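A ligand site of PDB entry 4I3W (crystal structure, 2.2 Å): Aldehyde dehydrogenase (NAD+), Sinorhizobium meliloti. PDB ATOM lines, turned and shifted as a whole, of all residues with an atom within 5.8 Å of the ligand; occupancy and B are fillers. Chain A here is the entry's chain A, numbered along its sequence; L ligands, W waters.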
ATOM      1  N   ILE A 157       3.054   0.478   7.408  1.00  0.00           N
ATOM      2  CA  ILE A 157       3.705   1.437   8.324  1.00  0.00           C
ATOM      3  C   ILE A 157       4.118   0.679   9.578  1.00  0.00           C
ATOM      4  O   ILE A 157       3.272   0.050  10.228  1.00  0.00           O
ATOM      5  CB  ILE A 157       2.749   2.588   8.696  1.00  0.00           C
ATOM      6  CG1 ILE A 157       2.332   3.351   7.426  1.00  0.00           C
ATOM      7  CG2 ILE A 157       3.394   3.552   9.647  1.00  0.00           C
ATOM      8  CD1 ILE A 157       1.087   4.264   7.628  1.00  0.00           C
ATOM      9  N   THR A 158       5.398   0.725   9.926  1.00  0.00           N
ATOM     10  CA  THR A 158       5.947  -0.173  10.944  1.00  0.00           C
ATOM     11  C   THR A 158       6.587   0.571  12.117  1.00  0.00           C
ATOM     12  O   THR A 158       7.044   1.696  11.995  1.00  0.00           O
ATOM     13  CB  THR A 158       6.981  -1.190  10.355  1.00  0.00           C
ATOM     14  OG1 THR A 158       8.043  -0.465   9.715  1.00  0.00           O
ATOM     15  CG2 THR A 158       6.357  -2.144   9.358  1.00  0.00           C
ATOM     16  N   PRO A 159       6.618  -0.077  13.281  1.00  0.00           N
ATOM     17  CA  PRO A 159       7.087   0.571  14.494  1.00  0.00           C
ATOM     18  C   PRO A 159       8.529   0.220  14.808  1.00  0.00           C
ATOM     19  O   PRO A 159       9.163  -0.593  14.078  1.00  0.00           O
ATOM     20  CB  PRO A 159       6.177  -0.016  15.543  1.00  0.00           C
ATOM     21  CG  PRO A 159       5.987  -1.434  15.093  1.00  0.00           C
ATOM     22  CD  PRO A 159       6.062  -1.405  13.563  1.00  0.00           C
ATOM     23  N   PHE A 160       9.061   0.795  15.878  1.00  0.00           N
ATOM     24  CA  PHE A 160      10.494   0.591  16.155  1.00  0.00           C
ATOM     25  C   PHE A 160      10.831  -0.714  16.853  1.00  0.00           C
ATOM     26  O   PHE A 160      11.977  -1.141  16.832  1.00  0.00           O
ATOM     27  CB  PHE A 160      11.010   1.774  16.995  1.00  0.00           C
ATOM     28  CG  PHE A 160      10.476   1.804  18.376  1.00  0.00           C
ATOM     29  CD1 PHE A 160      10.955   0.930  19.353  1.00  0.00           C
ATOM     30  CD2 PHE A 160       9.523   2.732  18.717  1.00  0.00           C
ATOM     31  CE1 PHE A 160      10.473   0.977  20.649  1.00  0.00           C
ATOM     32  CE2 PHE A 160       9.027   2.791  20.003  1.00  0.00           C
ATOM     33  CZ  PHE A 160       9.501   1.891  20.971  1.00  0.00           C
ATOM     34  N   ASN A 161       9.856  -1.376  17.484  1.00  0.00           N
ATOM     35  CA  ASN A 161      10.204  -2.477  18.394  1.00  0.00           C
ATOM     36  C   ASN A 161      10.629  -3.772  17.741  1.00  0.00           C
ATOM     37  O   ASN A 161      11.298  -4.590  18.374  1.00  0.00           O
ATOM     38  CB  ASN A 161       9.095  -2.717  19.439  1.00  0.00           C
ATOM     39  CG  ASN A 161       7.839  -3.352  18.820  1.00  0.00           C
ATOM     40  OD1 ASN A 161       7.366  -2.940  17.761  1.00  0.00           O
ATOM     41  ND2 ASN A 161       7.296  -4.368  19.476  1.00  0.00           N
ATOM     42  N   LYS A 184       6.892   2.316   4.903  1.00  0.00           N
ATOM     43  CA  LYS A 184       7.542   3.421   5.578  1.00  0.00           C
ATOM     44  C   LYS A 184       7.858   2.989   7.015  1.00  0.00           C
ATOM     45  O   LYS A 184       7.015   3.035   7.907  1.00  0.00           O
ATOM     46  CB  LYS A 184       6.689   4.695   5.599  1.00  0.00           C
ATOM     47  CG  LYS A 184       7.370   5.891   6.303  1.00  0.00           C
ATOM     48  CD  LYS A 184       6.394   6.885   6.962  1.00  0.00           C
ATOM     49  CE  LYS A 184       5.945   6.416   8.320  1.00  0.00           C
ATOM     50  NZ  LYS A 184       7.092   5.995   9.164  1.00  0.00           N
ATOM     51  N   PRO A 185       9.092   2.577   7.251  1.00  0.00           N
ATOM     52  CA  PRO A 185       9.470   2.255   8.638  1.00  0.00           C
ATOM     53  C   PRO A 185       9.530   3.508   9.465  1.00  0.00           C
ATOM     54  O   PRO A 185       9.568   4.637   8.931  1.00  0.00           O
ATOM     55  CB  PRO A 185      10.873   1.659   8.489  1.00  0.00           C
ATOM     56  CG  PRO A 185      11.402   2.262   7.192  1.00  0.00           C
ATOM     57  CD  PRO A 185      10.192   2.412   6.291  1.00  0.00           C
ATOM     58  N   THR A 186       9.539   3.342  10.780  1.00  0.00           N
ATOM     59  CA  THR A 186       9.734   4.476  11.686  1.00  0.00           C
ATOM     60  C   THR A 186      11.098   5.092  11.449  1.00  0.00           C
ATOM     61  O   THR A 186      12.062   4.380  11.179  1.00  0.00           O
ATOM     62  CB  THR A 186       9.631   4.069  13.171  1.00  0.00           C
ATOM     63  OG1 THR A 186      10.079   5.153  13.977  1.00  0.00           O
ATOM     64  CG2 THR A 186      10.512   2.851  13.471  1.00  0.00           C
ATOM     65  N   GLU A 187      11.147   6.420  11.572  1.00  0.00           N
ATOM     66  CA  GLU A 187      12.393   7.156  11.452  1.00  0.00           C
ATOM     67  C   GLU A 187      13.405   6.748  12.527  1.00  0.00           C
ATOM     68  O   GLU A 187      14.605   6.973  12.366  1.00  0.00           O
ATOM     69  CB  GLU A 187      12.127   8.674  11.488  1.00  0.00           C
ATOM     70  CG  GLU A 187      11.659   9.221  12.850  1.00  0.00           C
ATOM     71  CD  GLU A 187      10.167   9.014  13.111  1.00  0.00           C
ATOM     72  OE1 GLU A 187       9.436   8.301  12.340  1.00  0.00           O
ATOM     73  OE2 GLU A 187       9.673   9.575  14.114  1.00  0.00           O
ATOM     74  N   LEU A 188      12.936   6.149  13.626  1.00  0.00           N
ATOM     75  CA  LEU A 188      13.851   5.711  14.680  1.00  0.00           C
ATOM     76  C   LEU A 188      14.663   4.476  14.344  1.00  0.00           C
ATOM     77  O   LEU A 188      15.782   4.333  14.842  1.00  0.00           O
ATOM     78  CB  LEU A 188      13.088   5.451  15.982  1.00  0.00           C
ATOM     79  CG  LEU A 188      12.361   6.673  16.517  1.00  0.00           C
ATOM     80  CD1 LEU A 188      11.531   6.278  17.729  1.00  0.00           C
ATOM     81  CD2 LEU A 188      13.378   7.776  16.870  1.00  0.00           C
ATOM     82  N   PRO A 217       7.287  11.848   9.779  1.00  0.00           N
ATOM     83  CA  PRO A 217       5.853  11.630   9.642  1.00  0.00           C
ATOM     84  C   PRO A 217       5.157  12.886   9.083  1.00  0.00           C
ATOM     85  O   PRO A 217       4.221  12.748   8.325  1.00  0.00           O
ATOM     86  CB  PRO A 217       5.398  11.380  11.070  1.00  0.00           C
ATOM     87  CG  PRO A 217       6.640  10.866  11.768  1.00  0.00           C
ATOM     88  CD  PRO A 217       7.787  11.580  11.145  1.00  0.00           C
ATOM     89  N   ALA A 218       5.635  14.060   9.445  1.00  0.00           N
ATOM     90  CA  ALA A 218       5.007  15.318   8.995  1.00  0.00           C
ATOM     91  C   ALA A 218       5.058  15.491   7.495  1.00  0.00           C
ATOM     92  O   ALA A 218       4.160  16.082   6.898  1.00  0.00           O
ATOM     93  CB  ALA A 218       5.643  16.524   9.689  1.00  0.00           C
ATOM     94  N   GLY A 221       4.224  10.850   5.982  1.00  0.00           N
ATOM     95  CA  GLY A 221       3.267   9.992   6.661  1.00  0.00           C
ATOM     96  C   GLY A 221       1.865  10.083   6.090  1.00  0.00           C
ATOM     97  O   GLY A 221       1.191   9.065   5.918  1.00  0.00           O
ATOM     98  N   MET A 222       1.410  11.291   5.789  1.00  0.00           N
ATOM     99  CA  MET A 222       0.038  11.431   5.315  1.00  0.00           C
ATOM    100  C   MET A 222      -0.137  10.769   3.965  1.00  0.00           C
ATOM    101  O   MET A 222      -1.189  10.160   3.702  1.00  0.00           O
ATOM    102  CB  MET A 222      -0.387  12.903   5.291  1.00  0.00           C
ATOM    103  CG  MET A 222      -1.886  13.122   4.973  1.00  0.00           C
ATOM    104  SD  MET A 222      -3.017  12.315   6.210  1.00  0.00           S
ATOM    105  CE  MET A 222      -2.545  13.233   7.690  1.00  0.00           C
ATOM    106  N   ILE A 225      -1.053   7.240   3.963  1.00  0.00           N
ATOM    107  CA  ILE A 225      -2.424   6.996   4.436  1.00  0.00           C
ATOM    108  C   ILE A 225      -3.477   7.340   3.370  1.00  0.00           C
ATOM    109  O   ILE A 225      -4.517   6.707   3.309  1.00  0.00           O
ATOM    110  CB  ILE A 225      -2.719   7.874   5.693  1.00  0.00           C
ATOM    111  CG1 ILE A 225      -1.823   7.485   6.844  1.00  0.00           C
ATOM    112  CG2 ILE A 225      -4.146   7.773   6.117  1.00  0.00           C
ATOM    113  CD1 ILE A 225      -1.677   5.998   6.897  1.00  0.00           C
ATOM    114  N   PHE A 235      -0.901  -1.216   9.617  1.00  0.00           N
ATOM    115  CA  PHE A 235      -0.159  -0.402  10.545  1.00  0.00           C
ATOM    116  C   PHE A 235       0.033  -1.138  11.869  1.00  0.00           C
ATOM    117  O   PHE A 235      -0.877  -1.826  12.353  1.00  0.00           O
ATOM    118  CB  PHE A 235      -0.912   0.918  10.787  1.00  0.00           C
ATOM    119  CG  PHE A 235      -0.403   1.715  11.977  1.00  0.00           C
ATOM    120  CD1 PHE A 235       0.635   2.640  11.834  1.00  0.00           C
ATOM    121  CD2 PHE A 235      -0.977   1.561  13.244  1.00  0.00           C
ATOM    122  CE1 PHE A 235       1.102   3.382  12.929  1.00  0.00           C
ATOM    123  CE2 PHE A 235      -0.510   2.304  14.338  1.00  0.00           C
ATOM    124  CZ  PHE A 235       0.517   3.229  14.174  1.00  0.00           C
ATOM    125  N   THR A 236       1.202  -0.969  12.472  1.00  0.00           N
ATOM    126  CA  THR A 236       1.431  -1.419  13.819  1.00  0.00           C
ATOM    127  C   THR A 236       2.148  -0.287  14.517  1.00  0.00           C
ATOM    128  O   THR A 236       3.132   0.245  13.991  1.00  0.00           O
ATOM    129  CB  THR A 236       2.322  -2.670  13.821  1.00  0.00           C
ATOM    130  OG1 THR A 236       1.685  -3.715  13.087  1.00  0.00           O
ATOM    131  CG2 THR A 236       2.590  -3.153  15.235  1.00  0.00           C
ATOM    132  N   GLY A 237       1.688   0.063  15.709  1.00  0.00           N
ATOM    133  CA  GLY A 237       2.257   1.187  16.439  1.00  0.00           C
ATOM    134  C   GLY A 237       1.357   1.573  17.627  1.00  0.00           C
ATOM    135  O   GLY A 237       0.661   0.716  18.208  1.00  0.00           O
ATOM    136  N   SER A 238       1.355   2.851  17.974  1.00  0.00           N
ATOM    137  CA  SER A 238       0.661   3.340  19.178  1.00  0.00           C
ATOM    138  C   SER A 238      -0.818   3.651  18.918  1.00  0.00           C
ATOM    139  O   SER A 238      -1.216   3.871  17.760  1.00  0.00           O
ATOM    140  CB  SER A 238       1.353   4.623  19.656  1.00  0.00           C
ATOM    141  OG  SER A 238       1.030   5.697  18.775  1.00  0.00           O
ATOM    142  N   VAL A 239      -1.605   3.720  19.979  1.00  0.00           N
ATOM    143  CA  VAL A 239      -3.018   4.068  19.883  1.00  0.00           C
ATOM    144  C   VAL A 239      -3.252   5.430  19.214  1.00  0.00           C
ATOM    145  O   VAL A 239      -3.984   5.516  18.216  1.00  0.00           O
ATOM    146  CB  VAL A 239      -3.734   3.999  21.269  1.00  0.00           C
ATOM    147  CG1 VAL A 239      -5.192   4.422  21.148  1.00  0.00           C
ATOM    148  CG2 VAL A 239      -3.641   2.584  21.865  1.00  0.00           C
ATOM    149  N   VAL A 241      -1.501   7.300  17.222  1.00  0.00           N
ATOM    150  CA  VAL A 241      -1.189   7.302  15.806  1.00  0.00           C
ATOM    151  C   VAL A 241      -2.163   6.407  15.052  1.00  0.00           C
ATOM    152  O   VAL A 241      -2.647   6.749  13.960  1.00  0.00           O
ATOM    153  CB  VAL A 241       0.276   6.909  15.518  1.00  0.00           C
ATOM    154  CG1 VAL A 241       0.504   6.715  14.027  1.00  0.00           C
ATOM    155  CG2 VAL A 241       1.217   7.975  16.063  1.00  0.00           C
ATOM    156  N   GLY A 242      -2.486   5.265  15.636  1.00  0.00           N
ATOM    157  CA  GLY A 242      -3.488   4.380  15.069  1.00  0.00           C
ATOM    158  C   GLY A 242      -4.841   5.055  14.842  1.00  0.00           C
ATOM    159  O   GLY A 242      -5.443   4.857  13.774  1.00  0.00           O
ATOM    160  N   LEU A 244      -5.475   8.163  14.474  1.00  0.00           N
ATOM    161  CA  LEU A 244      -5.294   9.217  13.484  1.00  0.00           C
ATOM    162  C   LEU A 244      -5.341   8.603  12.077  1.00  0.00           C
ATOM    163  O   LEU A 244      -5.950   9.137  11.135  1.00  0.00           O
ATOM    164  CB  LEU A 244      -3.952   9.905  13.725  1.00  0.00           C
ATOM    165  CG  LEU A 244      -3.563  11.106  12.878  1.00  0.00           C
ATOM    166  CD1 LEU A 244      -3.304  12.308  13.796  1.00  0.00           C
ATOM    167  CD2 LEU A 244      -2.345  10.795  12.019  1.00  0.00           C
ATOM    168  N   ILE A 245      -4.696   7.462  11.945  1.00  0.00           N
ATOM    169  CA  ILE A 245      -4.714   6.768  10.667  1.00  0.00           C
ATOM    170  C   ILE A 245      -6.121   6.295  10.316  1.00  0.00           C
ATOM    171  O   ILE A 245      -6.546   6.426   9.173  1.00  0.00           O
ATOM    172  CB  ILE A 245      -3.756   5.563  10.679  1.00  0.00           C
ATOM    173  CG1 ILE A 245      -2.328   6.046  10.605  1.00  0.00           C
ATOM    174  CG2 ILE A 245      -4.057   4.615   9.532  1.00  0.00           C
ATOM    175  CD1 ILE A 245      -1.331   4.949  10.889  1.00  0.00           C
ATOM    176  N   PHE A 390       6.222   0.418  28.225  1.00  0.00           N
ATOM    177  CA  PHE A 390       6.892  -0.324  27.157  1.00  0.00           C
ATOM    178  C   PHE A 390       8.383  -0.557  27.478  1.00  0.00           C
ATOM    179  O   PHE A 390       9.244  -0.318  26.646  1.00  0.00           O
ATOM    180  CB  PHE A 390       6.780   0.464  25.842  1.00  0.00           C
ATOM    181  CG  PHE A 390       6.627  -0.383  24.624  1.00  0.00           C
ATOM    182  CD1 PHE A 390       5.614  -1.341  24.535  1.00  0.00           C
ATOM    183  CD2 PHE A 390       7.460  -0.188  23.527  1.00  0.00           C
ATOM    184  CE1 PHE A 390       5.471  -2.121  23.388  1.00  0.00           C
ATOM    185  CE2 PHE A 390       7.330  -0.969  22.352  1.00  0.00           C
ATOM    186  CZ  PHE A 390       6.332  -1.936  22.286  1.00  0.00           C
HETATM  187  P1  LIG L   1       4.013   5.088  16.714  1.00  0.00           P
HETATM  188  O1  LIG L   1       4.439   6.313  17.485  1.00  0.00           O
HETATM  189  O2  LIG L   1       2.518   5.210  16.646  1.00  0.00           O
HETATM  190  O3  LIG L   1       4.711   5.078  15.275  1.00  0.00           O
HETATM  191  C1  LIG L   1       4.562   3.898  14.504  1.00  0.00           C
HETATM  192  C2  LIG L   1       4.654   4.283  13.046  1.00  0.00           C
HETATM  193  O4  LIG L   1       3.670   5.244  12.738  1.00  0.00           O
HETATM  194  C3  LIG L   1       6.012   4.852  12.719  1.00  0.00           C
HETATM  195  O5  LIG L   1       6.393   4.405  11.471  1.00  0.00           O
HETATM  196  C4  LIG L   1       5.697   6.254  12.747  1.00  0.00           C
HETATM  197  O6  LIG L   1       6.628   6.993  12.054  1.00  0.00           O
HETATM  198  C5  LIG L   1       4.314   6.274  12.128  1.00  0.00           C
HETATM  199  N1  LIG L   1       3.646   7.555  12.277  1.00  0.00           N
HETATM  200  C6  LIG L   1       3.808   8.400  13.371  1.00  0.00           C
HETATM  201  N2  LIG L   1       3.062   9.504  13.178  1.00  0.00           N
HETATM  202  C7  LIG L   1       2.399   9.427  11.936  1.00  0.00           C
HETATM  203  C8  LIG L   1       1.528  10.294  11.249  1.00  0.00           C
HETATM  204  N3  LIG L   1       1.179  11.517  11.875  1.00  0.00           N
HETATM  205  N4  LIG L   1       1.042   9.892  10.049  1.00  0.00           N
HETATM  206  C9  LIG L   1       1.394   8.706   9.522  1.00  0.00           C
HETATM  207  N5  LIG L   1       2.238   7.846  10.149  1.00  0.00           N
HETATM  208  C10 LIG L   1       2.752   8.170  11.347  1.00  0.00           C
HETATM  209  O7  LIG L   1       4.324   3.713  17.458  1.00  0.00           O
HETATM  210  P2  LIG L   1       5.779   3.323  18.051  1.00  0.00           P
HETATM  211  O8  LIG L   1       5.604   2.023  18.810  1.00  0.00           O
HETATM  212  O9  LIG L   1       6.796   2.924  16.946  1.00  0.00           O
HETATM  213  O10 LIG L   1       6.308   4.583  18.901  1.00  0.00           O
HETATM  214  O   HOH W   1       8.530   8.146   9.902  1.00  0.00           O
HETATM  215  O   HOH W   2       8.083   5.710  16.050  1.00  0.00           O
HETATM  216  O   HOH W   3       7.425  -0.011  18.881  1.00  0.00           O
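O2 of the ligand sits at hydrogen-bond distance from N of Ser 238. O2 of the ligand lies within hydrogen-bond range of OG of Ser 238 (2.6 Å). O5 of the ligand is in hydrogen-bond range of O of Thr 158 (2.8 Å). NZ of Lys 184 lies within hydrogen-bond range of O5 of the ligand, at 2.9 Å. OE1 of Glu 187 lies within hydrogen-bond range of O6 of the ligand, 3.1 Å away. The backbone NH (N) of Phe 160 sits close to an oxygen (O9) of the ligand, at 3.3 Å. The backbone NH of Thr 186 sits close to an oxygen (O5) of the ligand (3.4 Å).
The side-chain hydroxyl (OG) of Ser 238 is in hydrogen-bond range of the backbone NH (N) of Val 241 (3.4 Å). The backbone carbonyl oxygen (O) of Lys 184 lies within hydrogen-bond range of the backbone NH (N) of Thr 158 (3.5 Å). O of Thr 158 lies within hydrogen-bond range of N of Thr 186, 3.2 Å away. OG1 of Thr 186 lies close to N of Leu 188 (3.0 Å). O of Ile 157 lies within hydrogen-bond range of N of Thr 236, 3.2 Å away.
CG2 of Ile 157 touches O4 of the ligand, at 3.5 Å. Pro 159 touches the ligand (CB to O9, 3.3 Å). Pro 185 touches the ligand (C to O5, 3.8 Å). Pro 217 touches the ligand (CB to N2, 3.7 Å). O of Gly 221 touches C9 of the ligand, 3.6 Å away. Phe 235 touches the ligand (CE1 to O4, 3.2 Å). Thr 236 touches the ligand. CA of Gly 237 touches O7 of the ligand (3.4 Å). CB of Val 241 touches O2 of the ligand, 3.0 Å away. Leu 244 touches the ligand. Hydrophobic or aromatic side chains within 4 Å of the ligand: Ile 157, Pro 159, Phe 160, Pro 217, Phe 235, Val 241 and Leu 244. 16 residues have an atom within 4 Å of the ligand: Ile 157, Thr 158, Pro 159, Phe 160, Lys 184, Pro 185, Thr 186, Glu 187, Pro 217, Gly 221, Phe 235, Thr 236, Gly 237, Ser 238, Val 241 and Leu 244. The nearest printed residue that does not touch the ligand is Ile 225 (4.4 Å).
Water W3 bridges O8 of the ligand (2.7 Å) and N of Asn 161 (3.1 Å). Water W1 lies within hydrogen-bond range of the side-chain carboxylate of Glu 187 (2.6 Å), the side-chain amino group of Lys 184 (2.7 Å) and an oxygen (O6) of the ligand (3.1 Å). Water W2 bridges the side-chain hydroxyl of Thr 186 (2.9 Å) and an oxygen (O9) of the ligand (3.2 Å).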
